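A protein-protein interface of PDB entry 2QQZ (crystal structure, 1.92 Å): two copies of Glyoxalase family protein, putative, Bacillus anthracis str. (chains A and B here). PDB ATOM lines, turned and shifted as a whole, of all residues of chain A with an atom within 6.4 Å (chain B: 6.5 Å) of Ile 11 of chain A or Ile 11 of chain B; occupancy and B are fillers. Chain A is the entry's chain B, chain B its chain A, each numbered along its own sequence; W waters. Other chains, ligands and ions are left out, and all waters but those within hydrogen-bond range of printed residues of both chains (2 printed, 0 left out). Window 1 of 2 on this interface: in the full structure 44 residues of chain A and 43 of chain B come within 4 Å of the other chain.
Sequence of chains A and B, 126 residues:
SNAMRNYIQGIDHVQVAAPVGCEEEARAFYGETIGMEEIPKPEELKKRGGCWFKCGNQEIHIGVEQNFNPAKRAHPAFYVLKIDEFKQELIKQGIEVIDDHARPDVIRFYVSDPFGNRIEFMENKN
O of Gly 10 of chain A lies within hydrogen-bond range of N of Tyr 79 of chain B, at 2.9 Å.
The side-chain amide nitrogen of Gln 58 of chain B sits close to the side-chain amide nitrogen of Gln 58 of chain A (3.5 Å).
The backbone NH (N) of Gln 9 of chain B is in hydrogen-bond range of the backbone carbonyl oxygen (O) of Tyr 79 of chain A, at 2.8 Å.
The backbone carbonyl oxygen (O) of Gly 10 of chain B sits at hydrogen-bond distance from the backbone NH (N) of Tyr 79 of chain A, at 2.9 Å.
The backbone carbonyl oxygen (O) of Ala 77 of chain B lies within hydrogen-bond range of the backbone NH (N) of Asp 12 of chain A (2.7 Å).
The backbone carbonyl oxygen (O) of Tyr 79 of chain B lies within hydrogen-bond range of the backbone NH (N) of Gln 9 of chain A (2.7 Å).
The backbone NH of Ile 11 of chain B sits at hydrogen-bond distance from the side-chain amide oxygen of Gln 58 of chain A (2.8 Å).
O of Ala 77 of chain A lies within hydrogen-bond range of N of Asp 12 of chain B, at 2.8 Å.
O of His 13 of chain B is in hydrogen-bond range of N of Ala 77 of chain A, 2.9 Å away.
The side-chain amide oxygen (OE1) of Gln 58 of chain B is in hydrogen-bond range of the backbone NH (N) of Ile 11 of chain A, at 2.8 Å.
The backbone NH (N) of Ala 77 of chain B sits at hydrogen-bond distance from the backbone carbonyl oxygen (O) of His 13 of chain A.
N of Val 14 of chain B is in hydrogen-bond range of O of Glu 59 of chain B (3.3 Å).
OD2 of Asp 12 of chain B is in hydrogen-bond range of ND1 of His 13 of chain B (2.7 Å).
OD2 of Asp 12 of chain A sits at hydrogen-bond distance from ND1 of His 13 of chain A, at 2.8 Å.
O of Asp 12 of chain A sits at hydrogen-bond distance from N of Glu 59 of chain A (3.2 Å).
O of Gln 58 of chain B sits close to SG of Cys 55 of chain B (3.8 Å).
N of Val 14 of chain A is in hydrogen-bond range of O of Glu 59 of chain A.
Among the printed residues, merely in contact across the chains: Gln 58 of chain A with Gly 10 of chain B, Gly 56 of chain A with Gln 9 of chain B, Gln 9 of chain A with Gly 56 of chain B, Val 14 of chain A with Val 14 of chain B, Gly 10 of chain A with Gln 58 of chain B, Phe 78 of chain A with Gly 10 of chain B, Gly 10 of chain A with Phe 78 of chain B, Gly 10 of chain A with Cys 55 of chain B, Cys 55 of chain A with Gly 10 of chain B, Ile 11 of chain A with Ala 77 of chain B, Ala 77 of chain A with Ile 11 of chain B, Ile 11 of chain A with Glu 59 of chain B, Ile 8 of chain A with Tyr 79 of chain B, Ile 8 of chain A with Cys 55 of chain B, Tyr 79 of chain A with Ile 8 of chain B, Glu 59 of chain A with Ile 11 of chain B, Phe 78 of chain A with Ile 11 of chain B, Ile 11 of chain A with Phe 78 of chain B, Cys 55 of chain A with Ile 8 of chain B, His 13 of chain A with Pro 76 of chain B, Asp 12 of chain A with Tyr 79 of chain B, Pro 76 of chain A with His 13 of chain B, Tyr 79 of chain A with Asp 12 of chain B, Val 14 of chain A with Ile 11 of chain B, Ile 11 of chain A with Val 14 of chain B and Ile 11 of chain A with Ile 11 of chain B.
Of the printed residues of chain B, Asp 12 of chain A touches Ala 77 (2.7 Å) and Tyr 79 (3.8 Å).
Of the printed residues of chain B, Ala 77 of chain A touches Ile 11, Asp 12 and His 13.
Printed residues of chain A within 4 Å of Ile 11 of chain B: Ile 11, Val 14, Gln 58, Glu 59, Ala 77 and Phe 78.
Of the printed residues of chain A, Asp 12 of chain B touches Ala 77 (2.8 Å) and Tyr 79 (3.8 Å).
Of the printed residues of chain A, Glu 59 of chain B touches Ile 11 (3.6 Å).
Printed residues of chain A within 4 Å of Phe 78 of chain B: Gly 10 (3.3 Å) and Ile 11 (3.7 Å).
Of the 17 printed residues of chain A, 15 touch a printed residue of chain B.
Of the 17 printed residues of chain B, 15 touch a printed residue of chain A.
Among the printed residues, no Asp or Glu carboxylate lies within 4 Å of a Lys or Arg side-chain nitrogen of the other chain.
Gly 10 of chain A touches Phe 78 of chain B, and with the chains exchanged Phe 78 of chain A touches Gly 10 of chain B.
Ile 11 of chain A touches Ala 77 of chain B, and with the chains exchanged Ala 77 of chain A touches Ile 11 of chain B.
Asp 12 of chain A touches Tyr 79 of chain B, and with the chains exchanged Tyr 79 of chain A touches Asp 12 of chain B.
Val 14 of chain B touches its own counterpart, Val 14 of chain A.
Positions printed for both chains: 8, 9, 10, 11, 12, 13, 14, 55, 56, 57, 58, 59, 60, 76, 77, 78 and 79.
Of the 37 pairs that touch across the chains among the printed residues, 37 have their exchanged pair printed and touching as well.
Water W1 lies within hydrogen-bond range of N of Asn 57 of chain A, O of Gln 9 of chain B and OE1 of Gln 58 of chain A.
Water W2 lies within hydrogen-bond range of O of Ile 11 of chain B (2.9 Å), OE1 of Gln 58 of chain A (3.1 Å) and NE2 of Gln 58 of chain B (3.3 Å).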
ATOM      1  N   ILE A   8      18.165 -16.408 -35.035  1.00  0.00           N
ATOM      2  CA  ILE A   8      17.642 -15.893 -33.749  1.00  0.00           C
ATOM      3  C   ILE A   8      17.365 -17.037 -32.817  1.00  0.00           C
ATOM      4  O   ILE A   8      16.647 -17.991 -33.158  1.00  0.00           O
ATOM      5  CB  ILE A   8      16.400 -14.984 -33.918  1.00  0.00           C
ATOM      6  CG1 ILE A   8      16.817 -13.732 -34.696  1.00  0.00           C
ATOM      7  CG2 ILE A   8      15.809 -14.619 -32.548  1.00  0.00           C
ATOM      8  CD1 ILE A   8      15.745 -13.066 -35.434  1.00  0.00           C
ATOM      9  N   GLN A   9      17.951 -16.966 -31.640  1.00  0.00           N
ATOM     10  CA  GLN A   9      17.927 -18.081 -30.716  1.00  0.00           C
ATOM     11  C   GLN A   9      16.969 -17.853 -29.557  1.00  0.00           C
ATOM     12  O   GLN A   9      16.586 -18.824 -28.919  1.00  0.00           O
ATOM     13  CB  GLN A   9      19.330 -18.313 -30.190  1.00  0.00           C
ATOM     14  CG  GLN A   9      20.330 -18.759 -31.322  1.00  0.00           C
ATOM     15  CD  GLN A   9      19.836 -20.006 -32.105  1.00  0.00           C
ATOM     16  OE1 GLN A   9      19.428 -21.015 -31.518  1.00  0.00           O
ATOM     17  NE2 GLN A   9      19.894 -19.942 -33.434  1.00  0.00           N
ATOM     18  N   GLY A  10      16.606 -16.603 -29.276  1.00  0.00           N
ATOM     19  CA  GLY A  10      15.656 -16.308 -28.209  1.00  0.00           C
ATOM     20  C   GLY A  10      15.816 -14.881 -27.760  1.00  0.00           C
ATOM     21  O   GLY A  10      16.624 -14.118 -28.351  1.00  0.00           O
ATOM     22  N   ILE A  11      15.090 -14.521 -26.701  1.00  0.00           N
ATOM     23  CA  ILE A  11      15.193 -13.176 -26.112  1.00  0.00           C
ATOM     24  C   ILE A  11      16.283 -13.234 -25.034  1.00  0.00           C
ATOM     25  O   ILE A  11      16.203 -14.073 -24.139  1.00  0.00           O
ATOM     26  CB  ILE A  11      13.858 -12.735 -25.455  1.00  0.00           C
ATOM     27  CG1 ILE A  11      12.771 -12.602 -26.508  1.00  0.00           C
ATOM     28  CG2 ILE A  11      14.029 -11.358 -24.785  1.00  0.00           C
ATOM     29  CD1 ILE A  11      11.256 -12.471 -25.951  1.00  0.00           C
ATOM     30  N   ASP A  12      17.313 -12.388 -25.138  1.00  0.00           N
ATOM     31  CA  ASP A  12      18.401 -12.395 -24.141  1.00  0.00           C
ATOM     32  C   ASP A  12      17.942 -11.539 -22.957  1.00  0.00           C
ATOM     33  O   ASP A  12      18.117 -11.903 -21.774  1.00  0.00           O
ATOM     34  CB  ASP A  12      19.675 -11.795 -24.729  1.00  0.00           C
ATOM     35  CG  ASP A  12      20.802 -11.774 -23.724  1.00  0.00           C
ATOM     36  OD1 ASP A  12      21.559 -12.739 -23.735  1.00  0.00           O
ATOM     37  OD2 ASP A  12      20.891 -10.840 -22.882  1.00  0.00           O
ATOM     38  N   HIS A  13      17.393 -10.372 -23.284  1.00  0.00           N
ATOM     39  CA  HIS A  13      16.929  -9.485 -22.243  1.00  0.00           C
ATOM     40  C   HIS A  13      15.980  -8.474 -22.833  1.00  0.00           C
ATOM     41  O   HIS A  13      15.806  -8.333 -24.079  1.00  0.00           O
ATOM     42  CB  HIS A  13      18.136  -8.794 -21.514  1.00  0.00           C
ATOM     43  CG  HIS A  13      18.900  -7.840 -22.384  1.00  0.00           C
ATOM     44  ND1 HIS A  13      19.999  -8.217 -23.120  1.00  0.00           N
ATOM     45  CD2 HIS A  13      18.743  -6.505 -22.600  1.00  0.00           C
ATOM     46  CE1 HIS A  13      20.496  -7.161 -23.749  1.00  0.00           C
ATOM     47  NE2 HIS A  13      19.724  -6.115 -23.479  1.00  0.00           N
ATOM     48  N   VAL A  14      15.290  -7.794 -21.928  1.00  0.00           N
ATOM     49  CA  VAL A  14      14.502  -6.659 -22.281  1.00  0.00           C
ATOM     50  C   VAL A  14      15.038  -5.483 -21.480  1.00  0.00           C
ATOM     51  O   VAL A  14      15.486  -5.605 -20.316  1.00  0.00           O
ATOM     52  CB  VAL A  14      13.002  -6.915 -22.045  1.00  0.00           C
ATOM     53  CG1 VAL A  14      12.178  -5.656 -22.277  1.00  0.00           C
ATOM     54  CG2 VAL A  14      12.530  -8.023 -22.945  1.00  0.00           C
ATOM     55  N   CYS A  55      16.129 -13.121 -14.414  1.00  0.00           N
ATOM     56  CA  CYS A  55      14.864 -13.914 -14.357  1.00  0.00           C
ATOM     57  C   CYS A  55      15.049 -15.119 -15.217  1.00  0.00           C
ATOM     58  O   CYS A  55      14.991 -14.992 -16.437  1.00  0.00           O
ATOM     59  CB  CYS A  55      13.678 -13.139 -14.962  1.00  0.00           C
ATOM     60  SG  CYS A  55      14.031 -12.075 -16.417  1.00  0.00           S
ATOM     61  N   GLY A  56      15.354 -16.267 -14.617  1.00  0.00           N
ATOM     62  CA  GLY A  56      15.567 -17.449 -15.377  1.00  0.00           C
ATOM     63  C   GLY A  56      16.776 -17.281 -16.232  1.00  0.00           C
ATOM     64  O   GLY A  56      17.761 -16.734 -15.770  1.00  0.00           O
ATOM     65  N   ASN A  57      16.721 -17.728 -17.479  1.00  0.00           N
ATOM     66  CA  ASN A  57      17.865 -17.543 -18.384  1.00  0.00           C
ATOM     67  C   ASN A  57      17.883 -16.184 -19.053  1.00  0.00           C
ATOM     68  O   ASN A  57      18.645 -15.964 -20.012  1.00  0.00           O
ATOM     69  CB  ASN A  57      17.899 -18.619 -19.488  1.00  0.00           C
ATOM     70  CG  ASN A  57      18.415 -19.936 -18.998  1.00  0.00           C
ATOM     71  OD1 ASN A  57      19.384 -19.992 -18.241  1.00  0.00           O
ATOM     72  ND2 ASN A  57      17.777 -21.015 -19.430  1.00  0.00           N
ATOM     73  N   GLN A  58      17.013 -15.282 -18.612  1.00  0.00           N
ATOM     74  CA  GLN A  58      16.903 -13.989 -19.259  1.00  0.00           C
ATOM     75  C   GLN A  58      17.224 -12.935 -18.223  1.00  0.00           C
ATOM     76  O   GLN A  58      17.418 -13.269 -17.043  1.00  0.00           O
ATOM     77  CB  GLN A  58      15.521 -13.750 -19.911  1.00  0.00           C
ATOM     78  CG  GLN A  58      15.235 -14.584 -21.131  1.00  0.00           C
ATOM     79  CD  GLN A  58      14.719 -15.943 -20.780  1.00  0.00           C
ATOM     80  OE1 GLN A  58      13.770 -16.066 -20.009  1.00  0.00           O
ATOM     81  NE2 GLN A  58      15.345 -16.982 -21.318  1.00  0.00           N
ATOM     82  N   GLU A  59      17.359 -11.689 -18.687  1.00  0.00           N
ATOM     83  CA  GLU A  59      17.538 -10.556 -17.791  1.00  0.00           C
ATOM     84  C   GLU A  59      16.567  -9.429 -18.100  1.00  0.00           C
ATOM     85  O   GLU A  59      16.006  -9.331 -19.171  1.00  0.00           O
ATOM     86  CB  GLU A  59      18.973  -9.987 -17.930  1.00  0.00           C
ATOM     87  CG  GLU A  59      20.054 -11.039 -17.619  1.00  0.00           C
ATOM     88  CD  GLU A  59      21.464 -10.684 -18.077  1.00  0.00           C
ATOM     89  OE1 GLU A  59      21.713  -9.729 -18.874  1.00  0.00           O
ATOM     90  OE2 GLU A  59      22.351 -11.459 -17.631  1.00  0.00           O
ATOM     91  N   ILE A  60      16.430  -8.537 -17.132  1.00  0.00           N
ATOM     92  CA  ILE A  60      15.773  -7.272 -17.362  1.00  0.00           C
ATOM     93  C   ILE A  60      16.776  -6.180 -16.950  1.00  0.00           C
ATOM     94  O   ILE A  60      17.389  -6.281 -15.874  1.00  0.00           O
ATOM     95  CB  ILE A  60      14.400  -7.156 -16.592  1.00  0.00           C
ATOM     96  CG1 ILE A  60      13.806  -5.742 -16.763  1.00  0.00           C
ATOM     97  CG2 ILE A  60      14.539  -7.506 -15.149  1.00  0.00           C
ATOM     98  CD1 ILE A  60      12.272  -5.677 -16.447  1.00  0.00           C
ATOM     99  N   PRO A  76       7.118  -6.335 -21.460  1.00  0.00           N
ATOM    100  CA  PRO A  76       7.507  -7.711 -21.279  1.00  0.00           C
ATOM    101  C   PRO A  76       6.506  -8.576 -20.487  1.00  0.00           C
ATOM    102  O   PRO A  76       5.821  -8.060 -19.621  1.00  0.00           O
ATOM    103  CB  PRO A  76       8.813  -7.579 -20.502  1.00  0.00           C
ATOM    104  CG  PRO A  76       8.622  -6.288 -19.695  1.00  0.00           C
ATOM    105  CD  PRO A  76       7.747  -5.408 -20.475  1.00  0.00           C
ATOM    106  N   ALA A  77       6.430  -9.891 -20.788  1.00  0.00           N
ATOM    107  CA  ALA A  77       5.588 -10.830 -20.058  1.00  0.00           C
ATOM    108  C   ALA A  77       6.492 -11.926 -19.446  1.00  0.00           C
ATOM    109  O   ALA A  77       7.242 -12.610 -20.170  1.00  0.00           O
ATOM    110  CB  ALA A  77       4.575 -11.453 -20.953  1.00  0.00           C
ATOM    111  N   PHE A  78       6.449 -12.046 -18.123  1.00  0.00           N
ATOM    112  CA  PHE A  78       7.280 -13.024 -17.384  1.00  0.00           C
ATOM    113  C   PHE A  78       6.427 -14.243 -17.070  1.00  0.00           C
ATOM    114  O   PHE A  78       5.232 -14.084 -16.720  1.00  0.00           O
ATOM    115  CB  PHE A  78       7.832 -12.435 -16.087  1.00  0.00           C
ATOM    116  CG  PHE A  78       8.700 -11.237 -16.324  1.00  0.00           C
ATOM    117  CD1 PHE A  78      10.034 -11.398 -16.690  1.00  0.00           C
ATOM    118  CD2 PHE A  78       8.166  -9.951 -16.244  1.00  0.00           C
ATOM    119  CE1 PHE A  78      10.839 -10.286 -16.962  1.00  0.00           C
ATOM    120  CE2 PHE A  78       8.982  -8.844 -16.525  1.00  0.00           C
ATOM    121  CZ  PHE A  78      10.298  -9.032 -16.897  1.00  0.00           C
ATOM    122  N   TYR A  79       7.035 -15.431 -17.223  1.00  0.00           N
ATOM    123  CA  TYR A  79       6.381 -16.675 -16.923  1.00  0.00           C
ATOM    124  C   TYR A  79       6.579 -16.878 -15.438  1.00  0.00           C
ATOM    125  O   TYR A  79       7.702 -16.771 -14.973  1.00  0.00           O
ATOM    126  CB  TYR A  79       6.982 -17.873 -17.684  1.00  0.00           C
ATOM    127  CG  TYR A  79       6.037 -19.041 -17.615  1.00  0.00           C
ATOM    128  CD1 TYR A  79       5.025 -19.192 -18.569  1.00  0.00           C
ATOM    129  CD2 TYR A  79       6.076 -19.938 -16.535  1.00  0.00           C
ATOM    130  CE1 TYR A  79       4.107 -20.272 -18.470  1.00  0.00           C
ATOM    131  CE2 TYR A  79       5.165 -20.998 -16.420  1.00  0.00           C
ATOM    132  CZ  TYR A  79       4.196 -21.158 -17.398  1.00  0.00           C
ATOM    133  OH  TYR A  79       3.280 -22.180 -17.310  1.00  0.00           O
ATOM    134  N   ILE B   8       9.364 -16.318 -10.496  1.00  0.00           N
ATOM    135  CA  ILE B   8       9.589 -15.909 -11.880  1.00  0.00           C
ATOM    136  C   ILE B   8      10.549 -16.840 -12.642  1.00  0.00           C
ATOM    137  O   ILE B   8      11.680 -17.061 -12.210  1.00  0.00           O
ATOM    138  CB  ILE B   8      10.069 -14.402 -12.011  1.00  0.00           C
ATOM    139  CG1 ILE B   8       9.009 -13.411 -11.471  1.00  0.00           C
ATOM    140  CG2 ILE B   8      10.399 -14.120 -13.478  1.00  0.00           C
ATOM    141  CD1 ILE B   8       9.441 -11.888 -11.475  1.00  0.00           C
ATOM    142  N   GLN B   9      10.113 -17.382 -13.779  1.00  0.00           N
ATOM    143  CA  GLN B   9      10.883 -18.401 -14.481  1.00  0.00           C
ATOM    144  C   GLN B   9      11.682 -17.894 -15.686  1.00  0.00           C
ATOM    145  O   GLN B   9      12.655 -18.545 -16.128  1.00  0.00           O
ATOM    146  CB  GLN B   9       9.942 -19.508 -14.904  1.00  0.00           C
ATOM    147  CG  GLN B   9       9.348 -20.280 -13.691  1.00  0.00           C
ATOM    148  CD  GLN B   9      10.408 -20.846 -12.726  1.00  0.00           C
ATOM    149  OE1 GLN B   9      11.388 -21.472 -13.129  1.00  0.00           O
ATOM    150  NE2 GLN B   9      10.194 -20.636 -11.444  1.00  0.00           N
ATOM    151  N   GLY B  10      11.293 -16.739 -16.213  1.00  0.00           N
ATOM    152  CA  GLY B  10      11.924 -16.229 -17.410  1.00  0.00           C
ATOM    153  C   GLY B  10      10.968 -15.288 -18.130  1.00  0.00           C
ATOM    154  O   GLY B  10       9.868 -15.011 -17.642  1.00  0.00           O
ATOM    155  N   ILE B  11      11.411 -14.755 -19.257  1.00  0.00           N
ATOM    156  CA  ILE B  11      10.538 -13.957 -20.133  1.00  0.00           C
ATOM    157  C   ILE B  11       9.798 -14.953 -21.034  1.00  0.00           C
ATOM    158  O   ILE B  11      10.413 -15.732 -21.741  1.00  0.00           O
ATOM    159  CB  ILE B  11      11.387 -12.954 -20.989  1.00  0.00           C
ATOM    160  CG1 ILE B  11      12.049 -11.962 -20.047  1.00  0.00           C
ATOM    161  CG2 ILE B  11      10.534 -12.198 -22.063  1.00  0.00           C
ATOM    162  CD1 ILE B  11      13.176 -11.123 -20.710  1.00  0.00           C
ATOM    163  N   ASP B  12       8.481 -14.940 -20.970  1.00  0.00           N
ATOM    164  CA  ASP B  12       7.701 -15.729 -21.881  1.00  0.00           C
ATOM    165  C   ASP B  12       7.655 -15.070 -23.277  1.00  0.00           C
ATOM    166  O   ASP B  12       7.829 -15.719 -24.302  1.00  0.00           O
ATOM    167  CB  ASP B  12       6.290 -15.907 -21.337  1.00  0.00           C
ATOM    168  CG  ASP B  12       5.416 -16.692 -22.277  1.00  0.00           C
ATOM    169  OD1 ASP B  12       5.401 -17.916 -22.169  1.00  0.00           O
ATOM    170  OD2 ASP B  12       4.778 -16.099 -23.153  1.00  0.00           O
ATOM    171  N   HIS B  13       7.419 -13.775 -23.297  1.00  0.00           N
ATOM    172  CA  HIS B  13       7.338 -13.067 -24.568  1.00  0.00           C
ATOM    173  C   HIS B  13       7.472 -11.585 -24.307  1.00  0.00           C
ATOM    174  O   HIS B  13       7.409 -11.145 -23.179  1.00  0.00           O
ATOM    175  CB  HIS B  13       6.000 -13.374 -25.357  1.00  0.00           C
ATOM    176  CG  HIS B  13       4.762 -12.842 -24.707  1.00  0.00           C
ATOM    177  ND1 HIS B  13       4.022 -13.590 -23.813  1.00  0.00           N
ATOM    178  CD2 HIS B  13       4.114 -11.666 -24.838  1.00  0.00           C
ATOM    179  CE1 HIS B  13       2.983 -12.886 -23.399  1.00  0.00           C
ATOM    180  NE2 HIS B  13       3.018 -11.710 -24.006  1.00  0.00           N
ATOM    181  N   VAL B  14       7.697 -10.830 -25.384  1.00  0.00           N
ATOM    182  CA  VAL B  14       7.610  -9.378 -25.366  1.00  0.00           C
ATOM    183  C   VAL B  14       6.503  -8.938 -26.321  1.00  0.00           C
ATOM    184  O   VAL B  14       6.314  -9.506 -27.414  1.00  0.00           O
ATOM    185  CB  VAL B  14       8.965  -8.689 -25.748  1.00  0.00           C
ATOM    186  CG1 VAL B  14       9.975  -8.952 -24.678  1.00  0.00           C
ATOM    187  CG2 VAL B  14       9.504  -9.181 -27.147  1.00  0.00           C
ATOM    188  N   CYS B  55      10.704 -17.063 -31.329  1.00  0.00           N
ATOM    189  CA  CYS B  55      12.180 -16.973 -31.219  1.00  0.00           C
ATOM    190  C   CYS B  55      12.698 -17.919 -30.132  1.00  0.00           C
ATOM    191  O   CYS B  55      12.618 -17.595 -28.923  1.00  0.00           O
ATOM    192  CB  CYS B  55      12.643 -15.534 -30.944  1.00  0.00           C
ATOM    193  SG  CYS B  55      11.628 -14.585 -29.806  1.00  0.00           S
ATOM    194  N   GLY B  56      13.171 -19.111 -30.512  1.00  0.00           N
ATOM    195  CA  GLY B  56      13.662 -20.005 -29.498  1.00  0.00           C
ATOM    196  C   GLY B  56      12.535 -20.354 -28.569  1.00  0.00           C
ATOM    197  O   GLY B  56      11.403 -20.594 -29.021  1.00  0.00           O
ATOM    198  N   ASN B  57      12.788 -20.366 -27.262  1.00  0.00           N
ATOM    199  CA  ASN B  57      11.705 -20.724 -26.322  1.00  0.00           C
ATOM    200  C   ASN B  57      10.836 -19.552 -26.018  1.00  0.00           C
ATOM    201  O   ASN B  57       9.975 -19.635 -25.119  1.00  0.00           O
ATOM    202  CB  ASN B  57      12.232 -21.274 -24.983  1.00  0.00           C
ATOM    203  CG  ASN B  57      12.656 -22.689 -25.074  1.00  0.00           C
ATOM    204  OD1 ASN B  57      12.045 -23.478 -25.782  1.00  0.00           O
ATOM    205  ND2 ASN B  57      13.736 -23.026 -24.388  1.00  0.00           N
ATOM    206  N   GLN B  58      11.093 -18.432 -26.706  1.00  0.00           N
ATOM    207  CA  GLN B  58      10.280 -17.250 -26.495  1.00  0.00           C
ATOM    208  C   GLN B  58       9.453 -16.878 -27.749  1.00  0.00           C
ATOM    209  O   GLN B  58       9.539 -17.548 -28.821  1.00  0.00           O
ATOM    210  CB  GLN B  58      11.154 -16.059 -26.027  1.00  0.00           C
ATOM    211  CG  GLN B  58      11.799 -16.212 -24.653  1.00  0.00           C
ATOM    212  CD  GLN B  58      13.067 -17.050 -24.696  1.00  0.00           C
ATOM    213  OE1 GLN B  58      13.936 -16.800 -25.510  1.00  0.00           O
ATOM    214  NE2 GLN B  58      13.182 -18.051 -23.813  1.00  0.00           N
ATOM    215  N   GLU B  59       8.620 -15.845 -27.589  1.00  0.00           N
ATOM    216  CA  GLU B  59       7.800 -15.302 -28.677  1.00  0.00           C
ATOM    217  C   GLU B  59       7.884 -13.783 -28.696  1.00  0.00           C
ATOM    218  O   GLU B  59       8.208 -13.164 -27.708  1.00  0.00           O
ATOM    219  CB  GLU B  59       6.311 -15.678 -28.505  1.00  0.00           C
ATOM    220  CG  GLU B  59       6.161 -17.167 -28.298  1.00  0.00           C
ATOM    221  CD  GLU B  59       4.758 -17.632 -27.913  1.00  0.00           C
ATOM    222  OE1 GLU B  59       3.863 -16.853 -27.462  1.00  0.00           O
ATOM    223  OE2 GLU B  59       4.557 -18.857 -28.059  1.00  0.00           O
ATOM    224  N   ILE B  60       7.584 -13.196 -29.845  1.00  0.00           N
ATOM    225  CA  ILE B  60       7.383 -11.756 -29.913  1.00  0.00           C
ATOM    226  C   ILE B  60       5.939 -11.585 -30.392  1.00  0.00           C
ATOM    227  O   ILE B  60       5.548 -12.237 -31.339  1.00  0.00           O
ATOM    228  CB  ILE B  60       8.449 -11.029 -30.830  1.00  0.00           C
ATOM    229  CG1 ILE B  60       8.252  -9.502 -30.765  1.00  0.00           C
ATOM    230  CG2 ILE B  60       8.382 -11.505 -32.287  1.00  0.00           C
ATOM    231  CD1 ILE B  60       9.253  -8.730 -31.576  1.00  0.00           C
ATOM    232  N   PRO B  76      13.383  -4.867 -26.688  1.00  0.00           N
ATOM    233  CA  PRO B  76      13.838  -6.237 -26.528  1.00  0.00           C
ATOM    234  C   PRO B  76      15.170  -6.493 -27.279  1.00  0.00           C
ATOM    235  O   PRO B  76      15.424  -5.910 -28.380  1.00  0.00           O
ATOM    236  CB  PRO B  76      12.694  -7.050 -27.183  1.00  0.00           C
ATOM    237  CG  PRO B  76      12.199  -6.069 -28.261  1.00  0.00           C
ATOM    238  CD  PRO B  76      12.301  -4.752 -27.686  1.00  0.00           C
ATOM    239  N   ALA B  77      15.971  -7.402 -26.698  1.00  0.00           N
ATOM    240  CA  ALA B  77      17.269  -7.804 -27.260  1.00  0.00           C
ATOM    241  C   ALA B  77      17.290  -9.323 -27.479  1.00  0.00           C
ATOM    242  O   ALA B  77      17.024 -10.110 -26.562  1.00  0.00           O
ATOM    243  CB  ALA B  77      18.447  -7.328 -26.399  1.00  0.00           C
ATOM    244  N   PHE B  78      17.533  -9.693 -28.736  1.00  0.00           N
ATOM    245  CA  PHE B  78      17.521 -11.084 -29.212  1.00  0.00           C
ATOM    246  C   PHE B  78      18.920 -11.611 -29.349  1.00  0.00           C
ATOM    247  O   PHE B  78      19.789 -10.921 -29.851  1.00  0.00           O
ATOM    248  CB  PHE B  78      16.811 -11.172 -30.552  1.00  0.00           C
ATOM    249  CG  PHE B  78      15.406 -10.733 -30.474  1.00  0.00           C
ATOM    250  CD1 PHE B  78      14.425 -11.615 -30.032  1.00  0.00           C
ATOM    251  CD2 PHE B  78      15.048  -9.448 -30.808  1.00  0.00           C
ATOM    252  CE1 PHE B  78      13.093 -11.207 -29.952  1.00  0.00           C
ATOM    253  CE2 PHE B  78      13.714  -9.037 -30.699  1.00  0.00           C
ATOM    254  CZ  PHE B  78      12.748  -9.916 -30.278  1.00  0.00           C
ATOM    255  N   TYR B  79      19.126 -12.827 -28.856  1.00  0.00           N
ATOM    256  CA  TYR B  79      20.414 -13.511 -28.977  1.00  0.00           C
ATOM    257  C   TYR B  79      20.451 -14.164 -30.356  1.00  0.00           C
ATOM    258  O   TYR B  79      19.462 -14.857 -30.769  1.00  0.00           O
ATOM    259  CB  TYR B  79      20.634 -14.553 -27.861  1.00  0.00           C
ATOM    260  CG  TYR B  79      22.111 -14.958 -27.788  1.00  0.00           C
ATOM    261  CD1 TYR B  79      22.981 -14.283 -26.925  1.00  0.00           C
ATOM    262  CD2 TYR B  79      22.651 -15.933 -28.646  1.00  0.00           C
ATOM    263  CE1 TYR B  79      24.328 -14.612 -26.861  1.00  0.00           C
ATOM    264  CE2 TYR B  79      24.045 -16.257 -28.602  1.00  0.00           C
ATOM    265  CZ  TYR B  79      24.847 -15.584 -27.685  1.00  0.00           C
ATOM    266  OH  TYR B  79      26.190 -15.827 -27.580  1.00  0.00           O
HETATM  267  O   HOH W   1      14.739 -18.743 -18.391  1.00  0.00           O
HETATM  268  O   HOH W   2      11.655 -18.181 -20.912  1.00  0.00           O
